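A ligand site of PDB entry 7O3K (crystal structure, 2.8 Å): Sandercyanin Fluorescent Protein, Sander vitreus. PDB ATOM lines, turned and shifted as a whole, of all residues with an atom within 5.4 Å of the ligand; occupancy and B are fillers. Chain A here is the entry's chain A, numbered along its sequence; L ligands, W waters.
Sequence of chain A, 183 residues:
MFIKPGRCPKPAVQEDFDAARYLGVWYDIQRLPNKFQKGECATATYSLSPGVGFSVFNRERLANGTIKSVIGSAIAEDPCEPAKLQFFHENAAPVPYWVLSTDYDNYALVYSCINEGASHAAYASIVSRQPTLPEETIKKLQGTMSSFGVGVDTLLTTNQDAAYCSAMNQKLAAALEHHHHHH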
ATOM      1  N   TRP A  26      -4.785  23.287 -27.561  1.00  0.00           N
ATOM      2  CA  TRP A  26      -5.635  24.464 -27.798  1.00  0.00           C
ATOM      3  C   TRP A  26      -4.842  25.671 -27.330  1.00  0.00           C
ATOM      4  O   TRP A  26      -4.303  25.630 -26.217  1.00  0.00           O
ATOM      5  CB  TRP A  26      -6.945  24.300 -27.020  1.00  0.00           C
ATOM      6  CG  TRP A  26      -7.990  23.436 -27.633  1.00  0.00           C
ATOM      7  CD1 TRP A  26      -8.283  22.141 -27.300  1.00  0.00           C
ATOM      8  CD2 TRP A  26      -8.933  23.806 -28.658  1.00  0.00           C
ATOM      9  NE1 TRP A  26      -9.332  21.686 -28.055  1.00  0.00           N
ATOM     10  CE2 TRP A  26      -9.751  22.690 -28.891  1.00  0.00           C
ATOM     11  CE3 TRP A  26      -9.168  24.977 -29.389  1.00  0.00           C
ATOM     12  CZ2 TRP A  26     -10.778  22.696 -29.830  1.00  0.00           C
ATOM     13  CZ3 TRP A  26     -10.172  24.985 -30.320  1.00  0.00           C
ATOM     14  CH2 TRP A  26     -10.969  23.861 -30.535  1.00  0.00           C
ATOM     15  N   TYR A  27      -4.720  26.702 -28.175  1.00  0.00           N
ATOM     16  CA  TYR A  27      -3.983  27.938 -27.809  1.00  0.00           C
ATOM     17  C   TYR A  27      -4.951  28.951 -27.213  1.00  0.00           C
ATOM     18  O   TYR A  27      -6.054  29.128 -27.725  1.00  0.00           O
ATOM     19  CB  TYR A  27      -3.308  28.560 -29.027  1.00  0.00           C
ATOM     20  CG  TYR A  27      -2.256  27.718 -29.686  1.00  0.00           C
ATOM     21  CD1 TYR A  27      -2.591  26.601 -30.439  1.00  0.00           C
ATOM     22  CD2 TYR A  27      -0.912  28.044 -29.576  1.00  0.00           C
ATOM     23  CE1 TYR A  27      -1.617  25.830 -31.051  1.00  0.00           C
ATOM     24  CE2 TYR A  27       0.068  27.278 -30.181  1.00  0.00           C
ATOM     25  CZ  TYR A  27      -0.290  26.173 -30.923  1.00  0.00           C
ATOM     26  OH  TYR A  27       0.665  25.406 -31.523  1.00  0.00           O
ATOM     27  N   ASP A  28      -4.511  29.610 -26.151  1.00  0.00           N
ATOM     28  CA  ASP A  28      -5.337  30.628 -25.514  1.00  0.00           C
ATOM     29  C   ASP A  28      -5.289  31.913 -26.333  1.00  0.00           C
ATOM     30  O   ASP A  28      -4.204  32.433 -26.625  1.00  0.00           O
ATOM     31  CB  ASP A  28      -4.877  30.895 -24.089  1.00  0.00           C
ATOM     32  CG  ASP A  28      -5.801  31.826 -23.332  1.00  0.00           C
ATOM     33  OD1 ASP A  28      -5.348  32.918 -22.918  1.00  0.00           O
ATOM     34  OD2 ASP A  28      -6.988  31.479 -23.169  1.00  0.00           O
ATOM     35  N   ASN A  34      -7.252  36.576 -13.782  1.00  0.00           N
ATOM     36  CA  ASN A  34      -7.469  35.719 -12.613  1.00  0.00           C
ATOM     37  C   ASN A  34      -6.153  35.581 -11.852  1.00  0.00           C
ATOM     38  O   ASN A  34      -5.113  36.125 -12.252  1.00  0.00           O
ATOM     39  CB  ASN A  34      -8.023  34.355 -13.016  1.00  0.00           C
ATOM     40  CG  ASN A  34      -7.092  33.602 -13.950  1.00  0.00           C
ATOM     41  OD1 ASN A  34      -6.063  34.121 -14.383  1.00  0.00           O
ATOM     42  ND2 ASN A  34      -7.455  32.359 -14.269  1.00  0.00           N
ATOM     43  N   PHE A  36      -4.426  32.672 -11.333  1.00  0.00           N
ATOM     44  CA  PHE A  36      -3.508  31.620 -11.749  1.00  0.00           C
ATOM     45  C   PHE A  36      -2.759  31.971 -13.026  1.00  0.00           C
ATOM     46  O   PHE A  36      -1.549  31.744 -13.114  1.00  0.00           O
ATOM     47  CB  PHE A  36      -4.274  30.305 -11.911  1.00  0.00           C
ATOM     48  CG  PHE A  36      -5.026  29.900 -10.669  1.00  0.00           C
ATOM     49  CD1 PHE A  36      -4.347  29.674  -9.480  1.00  0.00           C
ATOM     50  CD2 PHE A  36      -6.401  29.748 -10.694  1.00  0.00           C
ATOM     51  CE1 PHE A  36      -5.033  29.297  -8.337  1.00  0.00           C
ATOM     52  CE2 PHE A  36      -7.087  29.371  -9.551  1.00  0.00           C
ATOM     53  CZ  PHE A  36      -6.406  29.143  -8.376  1.00  0.00           C
ATOM     54  N   GLN A  37      -3.445  32.519 -14.028  1.00  0.00           N
ATOM     55  CA  GLN A  37      -2.817  32.813 -15.314  1.00  0.00           C
ATOM     56  C   GLN A  37      -2.190  34.205 -15.261  1.00  0.00           C
ATOM     57  O   GLN A  37      -2.778  35.212 -15.673  1.00  0.00           O
ATOM     58  CB  GLN A  37      -3.832  32.693 -16.456  1.00  0.00           C
ATOM     59  CG  GLN A  37      -4.815  31.541 -16.302  1.00  0.00           C
ATOM     60  CD  GLN A  37      -5.479  31.174 -17.614  1.00  0.00           C
ATOM     61  OE1 GLN A  37      -5.028  31.586 -18.688  1.00  0.00           O
ATOM     62  NE2 GLN A  37      -6.553  30.396 -17.539  1.00  0.00           N
ATOM     63  N   ALA A  42       0.173  30.831 -23.469  1.00  0.00           N
ATOM     64  CA  ALA A  42      -0.623  29.795 -22.780  1.00  0.00           C
ATOM     65  C   ALA A  42      -1.270  28.805 -23.721  1.00  0.00           C
ATOM     66  O   ALA A  42      -1.851  29.236 -24.733  1.00  0.00           O
ATOM     67  CB  ALA A  42      -1.671  30.466 -21.943  1.00  0.00           C
ATOM     68  N   THR A  43      -1.219  27.529 -23.363  1.00  0.00           N
ATOM     69  CA  THR A  43      -1.796  26.457 -24.150  1.00  0.00           C
ATOM     70  C   THR A  43      -2.424  25.422 -23.224  1.00  0.00           C
ATOM     71  O   THR A  43      -2.017  25.284 -22.070  1.00  0.00           O
ATOM     72  CB  THR A  43      -0.752  25.762 -25.040  1.00  0.00           C
ATOM     73  OG1 THR A  43       0.450  25.537 -24.289  1.00  0.00           O
ATOM     74  CG2 THR A  43      -0.424  26.623 -26.259  1.00  0.00           C
ATOM     75  N   ALA A  44      -3.413  24.710 -23.748  1.00  0.00           N
ATOM     76  CA  ALA A  44      -4.034  23.588 -23.045  1.00  0.00           C
ATOM     77  C   ALA A  44      -3.974  22.366 -23.950  1.00  0.00           C
ATOM     78  O   ALA A  44      -4.301  22.460 -25.140  1.00  0.00           O
ATOM     79  CB  ALA A  44      -5.474  23.899 -22.652  1.00  0.00           C
ATOM     80  N   TYR A  46      -5.292  18.424 -24.127  1.00  0.00           N
ATOM     81  CA  TYR A  46      -6.237  17.454 -23.574  1.00  0.00           C
ATOM     82  C   TYR A  46      -5.940  16.078 -24.156  1.00  0.00           C
ATOM     83  O   TYR A  46      -5.764  15.943 -25.377  1.00  0.00           O
ATOM     84  CB  TYR A  46      -7.674  17.876 -23.858  1.00  0.00           C
ATOM     85  CG  TYR A  46      -7.999  19.260 -23.330  1.00  0.00           C
ATOM     86  CD1 TYR A  46      -7.619  19.629 -22.049  1.00  0.00           C
ATOM     87  CD2 TYR A  46      -8.658  20.188 -24.123  1.00  0.00           C
ATOM     88  CE1 TYR A  46      -7.905  20.898 -21.564  1.00  0.00           C
ATOM     89  CE2 TYR A  46      -8.945  21.457 -23.638  1.00  0.00           C
ATOM     90  CZ  TYR A  46      -8.567  21.802 -22.354  1.00  0.00           C
ATOM     91  OH  TYR A  46      -8.855  23.058 -21.875  1.00  0.00           O
ATOM     92  N   ASN A  58      -1.968  22.270 -18.760  1.00  0.00           N
ATOM     93  CA  ASN A  58      -2.021  23.715 -19.080  1.00  0.00           C
ATOM     94  C   ASN A  58      -0.602  24.273 -18.934  1.00  0.00           C
ATOM     95  O   ASN A  58      -0.014  24.052 -17.876  1.00  0.00           O
ATOM     96  CB  ASN A  58      -3.058  24.410 -18.210  1.00  0.00           C
ATOM     97  CG  ASN A  58      -4.462  23.898 -18.398  1.00  0.00           C
ATOM     98  OD1 ASN A  58      -4.795  23.368 -19.456  1.00  0.00           O
ATOM     99  ND2 ASN A  58      -5.294  24.040 -17.383  1.00  0.00           N
ATOM    100  N   ARG A  59      -0.087  24.938 -19.963  1.00  0.00           N
ATOM    101  CA  ARG A  59       1.299  25.467 -19.931  1.00  0.00           C
ATOM    102  C   ARG A  59       1.331  26.948 -20.300  1.00  0.00           C
ATOM    103  O   ARG A  59       0.626  27.339 -21.229  1.00  0.00           O
ATOM    104  CB  ARG A  59       2.192  24.726 -20.927  1.00  0.00           C
ATOM    105  CG  ARG A  59       3.645  25.176 -20.898  1.00  0.00           C
ATOM    106  CD  ARG A  59       4.574  24.075 -21.363  1.00  0.00           C
ATOM    107  NE  ARG A  59       4.536  23.860 -22.804  1.00  0.00           N
ATOM    108  CZ  ARG A  59       5.436  24.319 -23.655  1.00  0.00           C
ATOM    109  NH1 ARG A  59       6.464  25.034 -23.221  1.00  0.00           N
ATOM    110  NH2 ARG A  59       5.310  24.074 -24.949  1.00  0.00           N
ATOM    111  N   GLU A  60       2.140  27.727 -19.585  1.00  0.00           N
ATOM    112  CA  GLU A  60       2.308  29.164 -19.907  1.00  0.00           C
ATOM    113  C   GLU A  60       3.730  29.582 -19.603  1.00  0.00           C
ATOM    114  O   GLU A  60       4.370  28.941 -18.763  1.00  0.00           O
ATOM    115  CB  GLU A  60       1.340  30.041 -19.124  1.00  0.00           C
ATOM    116  CG  GLU A  60       1.826  30.454 -17.741  1.00  0.00           C
ATOM    117  CD  GLU A  60       0.798  31.252 -16.958  1.00  0.00           C
ATOM    118  OE1 GLU A  60      -0.110  31.824 -17.580  1.00  0.00           O
ATOM    119  OE2 GLU A  60       0.900  31.289 -15.713  1.00  0.00           O
ATOM    120  N   LEU A  62       6.156  32.585 -18.172  1.00  0.00           N
ATOM    121  CA  LEU A  62       6.003  33.742 -17.278  1.00  0.00           C
ATOM    122  C   LEU A  62       6.920  34.867 -17.735  1.00  0.00           C
ATOM    123  O   LEU A  62       7.749  34.644 -18.623  1.00  0.00           O
ATOM    124  CB  LEU A  62       6.336  33.281 -15.859  1.00  0.00           C
ATOM    125  CG  LEU A  62       5.446  32.181 -15.297  1.00  0.00           C
ATOM    126  CD1 LEU A  62       6.045  31.615 -14.026  1.00  0.00           C
ATOM    127  CD2 LEU A  62       4.042  32.691 -15.046  1.00  0.00           C
ATOM    128  N   LYS A  68       5.728  27.514 -16.522  1.00  0.00           N
ATOM    129  CA  LYS A  68       5.060  26.851 -15.412  1.00  0.00           C
ATOM    130  C   LYS A  68       3.833  26.115 -15.931  1.00  0.00           C
ATOM    131  O   LYS A  68       3.024  26.699 -16.655  1.00  0.00           O
ATOM    132  CB  LYS A  68       4.662  27.867 -14.331  1.00  0.00           C
ATOM    133  CG  LYS A  68       4.349  27.262 -12.971  1.00  0.00           C
ATOM    134  CD  LYS A  68       3.632  28.272 -12.088  1.00  0.00           C
ATOM    135  CE  LYS A  68       2.945  27.613 -10.909  1.00  0.00           C
ATOM    136  NZ  LYS A  68       2.977  26.134 -10.994  1.00  0.00           N
ATOM    137  N   SER A  69       3.701  24.849 -15.546  1.00  0.00           N
ATOM    138  CA  SER A  69       2.597  24.008 -15.996  1.00  0.00           C
ATOM    139  C   SER A  69       1.819  23.488 -14.802  1.00  0.00           C
ATOM    140  O   SER A  69       2.294  23.474 -13.670  1.00  0.00           O
ATOM    141  CB  SER A  69       3.109  22.826 -16.834  1.00  0.00           C
ATOM    142  OG  SER A  69       4.073  23.243 -17.780  1.00  0.00           O
ATOM    143  N   VAL A  70       0.570  23.089 -15.074  1.00  0.00           N
ATOM    144  CA  VAL A  70      -0.264  22.391 -14.094  1.00  0.00           C
ATOM    145  C   VAL A  70      -0.880  21.168 -14.782  1.00  0.00           C
ATOM    146  O   VAL A  70      -1.190  21.202 -15.976  1.00  0.00           O
ATOM    147  CB  VAL A  70      -1.363  23.289 -13.491  1.00  0.00           C
ATOM    148  CG1 VAL A  70      -0.805  24.661 -13.110  1.00  0.00           C
ATOM    149  CG2 VAL A  70      -2.553  23.447 -14.438  1.00  0.00           C
ATOM    150  N   PHE A  87     -13.245  20.554 -13.395  1.00  0.00           N
ATOM    151  CA  PHE A  87     -11.763  20.522 -13.483  1.00  0.00           C
ATOM    152  C   PHE A  87     -11.174  20.227 -12.105  1.00  0.00           C
ATOM    153  O   PHE A  87     -11.306  21.064 -11.196  1.00  0.00           O
ATOM    154  CB  PHE A  87     -11.233  21.841 -14.052  1.00  0.00           C
ATOM    155  CG  PHE A  87      -9.736  21.988 -13.980  1.00  0.00           C
ATOM    156  CD1 PHE A  87      -8.903  21.062 -14.580  1.00  0.00           C
ATOM    157  CD2 PHE A  87      -9.164  23.055 -13.315  1.00  0.00           C
ATOM    158  CE1 PHE A  87      -7.530  21.188 -14.508  1.00  0.00           C
ATOM    159  CE2 PHE A  87      -7.779  23.188 -13.243  1.00  0.00           C
ATOM    160  CZ  PHE A  87      -6.976  22.257 -13.844  1.00  0.00           C
ATOM    161  N   HIS A  89      -7.754  19.567  -9.841  1.00  0.00           N
ATOM    162  CA  HIS A  89      -6.286  19.784  -9.861  1.00  0.00           C
ATOM    163  C   HIS A  89      -5.681  19.578  -8.480  1.00  0.00           C
ATOM    164  O   HIS A  89      -6.405  19.726  -7.500  1.00  0.00           O
ATOM    165  CB  HIS A  89      -5.917  21.146 -10.471  1.00  0.00           C
ATOM    166  CG  HIS A  89      -6.421  22.326  -9.725  1.00  0.00           C
ATOM    167  ND1 HIS A  89      -7.769  22.600  -9.598  1.00  0.00           N
ATOM    168  CD2 HIS A  89      -5.774  23.314  -9.084  1.00  0.00           C
ATOM    169  CE1 HIS A  89      -7.932  23.701  -8.905  1.00  0.00           C
ATOM    170  NE2 HIS A  89      -6.717  24.162  -8.575  1.00  0.00           N
ATOM    171  N   GLU A  90      -4.386  19.299  -8.431  1.00  0.00           N
ATOM    172  CA  GLU A  90      -3.712  18.979  -7.177  1.00  0.00           C
ATOM    173  C   GLU A  90      -3.895  20.059  -6.124  1.00  0.00           C
ATOM    174  O   GLU A  90      -3.585  21.234  -6.351  1.00  0.00           O
ATOM    175  CB  GLU A  90      -2.215  18.786  -7.477  1.00  0.00           C
ATOM    176  CG  GLU A  90      -1.989  18.204  -8.869  1.00  0.00           C
ATOM    177  CD  GLU A  90      -0.533  17.983  -9.203  1.00  0.00           C
ATOM    178  OE1 GLU A  90       0.319  18.727  -8.659  1.00  0.00           O
ATOM    179  OE2 GLU A  90      -0.244  17.078 -10.009  1.00  0.00           O
ATOM    180  N   VAL A  95     -13.266  23.192  -9.891  1.00  0.00           N
ATOM    181  CA  VAL A  95     -14.009  24.319 -10.442  1.00  0.00           C
ATOM    182  C   VAL A  95     -14.710  23.860 -11.706  1.00  0.00           C
ATOM    183  O   VAL A  95     -14.234  22.924 -12.370  1.00  0.00           O
ATOM    184  CB  VAL A  95     -13.072  25.512 -10.728  1.00  0.00           C
ATOM    185  CG1 VAL A  95     -12.449  26.027  -9.435  1.00  0.00           C
ATOM    186  CG2 VAL A  95     -11.994  25.125 -11.728  1.00  0.00           C
ATOM    187  N   PRO A  96     -15.846  24.452 -12.071  1.00  0.00           N
ATOM    188  CA  PRO A  96     -16.572  23.994 -13.259  1.00  0.00           C
ATOM    189  C   PRO A  96     -15.775  24.243 -14.538  1.00  0.00           C
ATOM    190  O   PRO A  96     -14.896  25.113 -14.599  1.00  0.00           O
ATOM    191  CB  PRO A  96     -17.855  24.815 -13.232  1.00  0.00           C
ATOM    192  CG  PRO A  96     -17.988  25.300 -11.825  1.00  0.00           C
ATOM    193  CD  PRO A  96     -16.585  25.489 -11.344  1.00  0.00           C
ATOM    194  N   TYR A  97     -16.099  23.460 -15.556  1.00  0.00           N
ATOM    195  CA  TYR A  97     -15.508  23.598 -16.886  1.00  0.00           C
ATOM    196  C   TYR A  97     -16.633  23.340 -17.893  1.00  0.00           C
ATOM    197  O   TYR A  97     -16.959  22.191 -18.188  1.00  0.00           O
ATOM    198  CB  TYR A  97     -14.340  22.633 -17.086  1.00  0.00           C
ATOM    199  CG  TYR A  97     -13.577  22.824 -18.388  1.00  0.00           C
ATOM    200  CD1 TYR A  97     -14.085  22.366 -19.594  1.00  0.00           C
ATOM    201  CD2 TYR A  97     -12.339  23.450 -18.396  1.00  0.00           C
ATOM    202  CE1 TYR A  97     -13.388  22.532 -20.782  1.00  0.00           C
ATOM    203  CE2 TYR A  97     -11.626  23.616 -19.569  1.00  0.00           C
ATOM    204  CZ  TYR A  97     -12.160  23.159 -20.756  1.00  0.00           C
ATOM    205  OH  TYR A  97     -11.464  23.327 -21.930  1.00  0.00           O
ATOM    206  N   VAL A 110     -15.003  28.440 -23.555  1.00  0.00           N
ATOM    207  CA  VAL A 110     -15.118  27.767 -22.269  1.00  0.00           C
ATOM    208  C   VAL A 110     -15.468  28.783 -21.198  1.00  0.00           C
ATOM    209  O   VAL A 110     -14.896  29.877 -21.154  1.00  0.00           O
ATOM    210  CB  VAL A 110     -13.819  27.007 -21.916  1.00  0.00           C
ATOM    211  CG1 VAL A 110     -14.044  26.106 -20.712  1.00  0.00           C
ATOM    212  CG2 VAL A 110     -13.316  26.211 -23.108  1.00  0.00           C
ATOM    213  N   TYR A 111     -16.401  28.415 -20.321  1.00  0.00           N
ATOM    214  CA  TYR A 111     -16.835  29.275 -19.226  1.00  0.00           C
ATOM    215  C   TYR A 111     -16.765  28.497 -17.923  1.00  0.00           C
ATOM    216  O   TYR A 111     -16.846  27.269 -17.891  1.00  0.00           O
ATOM    217  CB  TYR A 111     -18.253  29.810 -19.454  1.00  0.00           C
ATOM    218  CG  TYR A 111     -18.716  30.796 -18.402  1.00  0.00           C
ATOM    219  CD1 TYR A 111     -18.154  32.058 -18.299  1.00  0.00           C
ATOM    220  CD2 TYR A 111     -19.724  30.462 -17.500  1.00  0.00           C
ATOM    221  CE1 TYR A 111     -18.564  32.962 -17.338  1.00  0.00           C
ATOM    222  CE2 TYR A 111     -20.148  31.348 -16.531  1.00  0.00           C
ATOM    223  CZ  TYR A 111     -19.567  32.604 -16.454  1.00  0.00           C
ATOM    224  OH  TYR A 111     -19.984  33.491 -15.505  1.00  0.00           O
ATOM    225  N   SER A 112     -16.633  29.249 -16.829  1.00  0.00           N
ATOM    226  CA  SER A 112     -16.579  28.679 -15.488  1.00  0.00           C
ATOM    227  C   SER A 112     -16.972  29.760 -14.495  1.00  0.00           C
ATOM    228  O   SER A 112     -16.536  30.898 -14.613  1.00  0.00           O
ATOM    229  CB  SER A 112     -15.176  28.143 -15.161  1.00  0.00           C
ATOM    230  OG  SER A 112     -15.134  27.566 -13.877  1.00  0.00           O
ATOM    231  N   TYR A 123     -14.106  32.274 -14.747  1.00  0.00           N
ATOM    232  CA  TYR A 123     -13.089  32.148 -15.778  1.00  0.00           C
ATOM    233  C   TYR A 123     -13.784  32.091 -17.133  1.00  0.00           C
ATOM    234  O   TYR A 123     -14.918  31.616 -17.232  1.00  0.00           O
ATOM    235  CB  TYR A 123     -12.213  30.893 -15.598  1.00  0.00           C
ATOM    236  CG  TYR A 123     -11.639  30.684 -14.206  1.00  0.00           C
ATOM    237  CD1 TYR A 123     -12.427  30.196 -13.169  1.00  0.00           C
ATOM    238  CD2 TYR A 123     -10.303  30.966 -13.945  1.00  0.00           C
ATOM    239  CE1 TYR A 123     -11.895  30.007 -11.912  1.00  0.00           C
ATOM    240  CE2 TYR A 123      -9.772  30.777 -12.688  1.00  0.00           C
ATOM    241  CZ  TYR A 123     -10.568  30.291 -11.674  1.00  0.00           C
ATOM    242  OH  TYR A 123     -10.037  30.102 -10.416  1.00  0.00           O
ATOM    243  N   ALA A 124     -13.102  32.581 -18.157  1.00  0.00           N
ATOM    244  CA  ALA A 124     -13.611  32.507 -19.523  1.00  0.00           C
ATOM    245  C   ALA A 124     -12.415  32.495 -20.470  1.00  0.00           C
ATOM    246  O   ALA A 124     -11.409  33.162 -20.217  1.00  0.00           O
ATOM    247  CB  ALA A 124     -14.540  33.681 -19.852  1.00  0.00           C
ATOM    248  N   SER A 125     -12.536  31.740 -21.555  1.00  0.00           N
ATOM    249  CA  SER A 125     -11.397  31.537 -22.435  1.00  0.00           C
ATOM    250  C   SER A 125     -11.848  31.342 -23.871  1.00  0.00           C
ATOM    251  O   SER A 125     -12.717  30.511 -24.159  1.00  0.00           O
ATOM    252  CB  SER A 125     -10.572  30.330 -21.988  1.00  0.00           C
ATOM    253  OG  SER A 125      -9.377  30.218 -22.741  1.00  0.00           O
ATOM    254  N   VAL A 127     -10.257  29.858 -27.086  1.00  0.00           N
ATOM    255  CA  VAL A 127      -9.128  29.024 -27.453  1.00  0.00           C
ATOM    256  C   VAL A 127      -9.205  28.688 -28.930  1.00  0.00           C
ATOM    257  O   VAL A 127     -10.288  28.605 -29.523  1.00  0.00           O
ATOM    258  CB  VAL A 127      -9.052  27.732 -26.602  1.00  0.00           C
ATOM    259  CG1 VAL A 127      -8.667  28.064 -25.171  1.00  0.00           C
ATOM    260  CG2 VAL A 127     -10.380  26.992 -26.633  1.00  0.00           C
HETATM  261  C1  LIG L   1      -4.031  27.171 -14.330  1.00  0.00           C
HETATM  262  N1  LIG L   1      -6.446  26.981 -14.550  1.00  0.00           N
HETATM  263  C2  LIG L   1      -5.368  26.954 -13.739  1.00  0.00           C
HETATM  264  C3  LIG L   1      -5.681  26.689 -12.296  1.00  0.00           C
HETATM  265  C4  LIG L   1      -7.152  26.567 -12.319  1.00  0.00           C
HETATM  266  C5  LIG L   1      -7.513  26.768 -13.751  1.00  0.00           C
HETATM  267  C6  LIG L   1      -8.096  26.292 -11.177  1.00  0.00           C
HETATM  268  C7  LIG L   1      -4.803  26.572 -11.049  1.00  0.00           C
HETATM  269  C8  LIG L   1      -3.306  26.750 -11.284  1.00  0.00           C
HETATM  270  C9  LIG L   1      -2.482  26.199 -10.148  1.00  0.00           C
HETATM  271  O1  LIG L   1      -1.386  26.730  -9.895  1.00  0.00           O
HETATM  272  O2  LIG L   1      -2.934  25.226  -9.504  1.00  0.00           O
HETATM  273  C10 LIG L   1      -8.890  26.708 -14.293  1.00  0.00           C
HETATM  274  N2  LIG L   1      -8.613  28.208 -16.224  1.00  0.00           N
HETATM  275  C11 LIG L   1      -9.412  27.399 -15.490  1.00  0.00           C
HETATM  276  C12 LIG L   1     -10.818  27.289 -15.977  1.00  0.00           C
HETATM  277  C13 LIG L   1     -10.795  28.162 -17.171  1.00  0.00           C
HETATM  278  C14 LIG L   1      -9.404  28.668 -17.214  1.00  0.00           C
HETATM  279  C15 LIG L   1     -11.927  26.460 -15.366  1.00  0.00           C
HETATM  280  O3  LIG L   1      -9.001  29.479 -18.131  1.00  0.00           O
HETATM  281  C16 LIG L   1     -11.882  28.501 -18.131  1.00  0.00           C
HETATM  282  C17 LIG L   1     -13.117  28.050 -18.006  1.00  0.00           C
HETATM  283  N3  LIG L   1      -6.763  26.828 -18.579  1.00  0.00           N
HETATM  284  C18 LIG L   1      -7.931  26.560 -19.230  1.00  0.00           C
HETATM  285  C19 LIG L   1      -7.994  26.969 -20.662  1.00  0.00           C
HETATM  286  C20 LIG L   1      -6.642  27.546 -20.819  1.00  0.00           C
HETATM  287  C21 LIG L   1      -5.982  27.416 -19.503  1.00  0.00           C
HETATM  288  C22 LIG L   1      -9.112  26.832 -21.666  1.00  0.00           C
HETATM  289  O4  LIG L   1      -8.916  25.991 -18.642  1.00  0.00           O
HETATM  290  C23 LIG L   1      -6.056  28.154 -22.041  1.00  0.00           C
HETATM  291  C24 LIG L   1      -5.634  27.389 -23.030  1.00  0.00           C
HETATM  292  C25 LIG L   1      -4.609  27.869 -19.179  1.00  0.00           C
HETATM  293  N4  LIG L   1      -4.646  27.483 -16.718  1.00  0.00           N
HETATM  294  C26 LIG L   1      -3.952  27.714 -17.860  1.00  0.00           C
HETATM  295  C27 LIG L   1      -2.488  27.819 -17.676  1.00  0.00           C
HETATM  296  C28 LIG L   1      -2.304  27.617 -16.230  1.00  0.00           C
HETATM  297  C29 LIG L   1      -3.692  27.419 -15.754  1.00  0.00           C
HETATM  298  C30 LIG L   1      -1.455  28.078 -18.736  1.00  0.00           C
HETATM  299  C31 LIG L   1      -1.021  27.598 -15.418  1.00  0.00           C
HETATM  300  C32 LIG L   1      -0.973  28.831 -14.520  1.00  0.00           C
HETATM  301  C33 LIG L   1       0.305  28.821 -13.710  1.00  0.00           C
HETATM  302  O5  LIG L   1       0.217  28.779 -12.461  1.00  0.00           O
HETATM  303  O6  LIG L   1       1.395  28.842 -14.319  1.00  0.00           O
HETATM  304  O   HOH W   1      -7.650  23.527 -19.386  1.00  0.00           O
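NE2 of Gln 37 sits at hydrogen-bond distance from O3 of the ligand, 2.7 Å away.
The side-chain carboxylate (OE2) of Glu 60 sits close to an oxygen (O6) of the ligand, 2.9 Å away.
A nitrogen (N3) of the ligand sits close to the side-chain amide nitrogen (ND2) of Asn 58 (3.4 Å).
Water W1 lies within hydrogen-bond range of the side-chain hydroxyl (OH) of Tyr 46, the side-chain amide oxygen (OD1) of Asn 58 and an oxygen (O4) of the ligand.
The backbone carbonyl oxygen (O) of Glu 60 sits at hydrogen-bond distance from the backbone NH (N) of Lys 68, at 3.0 Å.
The backbone carbonyl oxygen (O) of Arg 59 lies within hydrogen-bond range of the backbone NH (N) of Thr 43 (2.8 Å).
O of Pro 96 lies within hydrogen-bond range of OG of Ser 112, 2.6 Å away.
The backbone carbonyl oxygen (O) of Asn 58 is in hydrogen-bond range of the backbone NH (N) of Val 70 (3.0 Å).
O of Ser 112 sits at hydrogen-bond distance from N of Tyr 123.
N of Ser 125 is in hydrogen-bond range of O of Val 110.
N of Trp 26 lies within hydrogen-bond range of O of Ala 44 (2.6 Å).
N of Asp 28 sits at hydrogen-bond distance from O of Ala 42 (3.0 Å).
O of Trp 26 touches C24 of the ligand, 3.9 Å away.
Asp 28 touches the ligand (CB to C23, 3.6 Å).
Phe 36 touches the ligand.
Thr 43 touches the ligand.
Ala 44 touches the ligand (CB to C24, 3.5 Å).
Tyr 46 touches the ligand.
O of Arg 59 touches C30 of the ligand (3.3 Å).
Lys 68 touches the ligand.
Val 70 touches the ligand.
Phe 87 touches the ligand.
CD2 of His 89 touches O2 of the ligand (3.4 Å).
CG2 of Val 95 touches C15 of the ligand, at 3.9 Å.
O of Pro 96 touches C15 of the ligand, 3.3 Å away.
Tyr 97 touches the ligand.
Val 110 touches the ligand (CG1 to C17, 3.5 Å).
C of Tyr 111 touches C17 of the ligand (3.7 Å).
CB of Ser 112 touches C17 of the ligand, 3.5 Å away.
Tyr 123 touches the ligand.
Ser 125 touches the ligand (OG to C22, 3.6 Å).
Val 127 touches the ligand (CG1 to C22, 3.7 Å).
Hydrophobic or aromatic side chains within 4 Å of the ligand: Phe 36, Ala 44, Val 70, Phe 87, His 89, Val 95, Tyr 97, Val 110, Tyr 123 and Val 127.
Along chain A the residues within 4 Å of the ligand span positions 26 to 127.
The nearest printed residue that does not touch the ligand is Ala 42 (4.004 Å).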
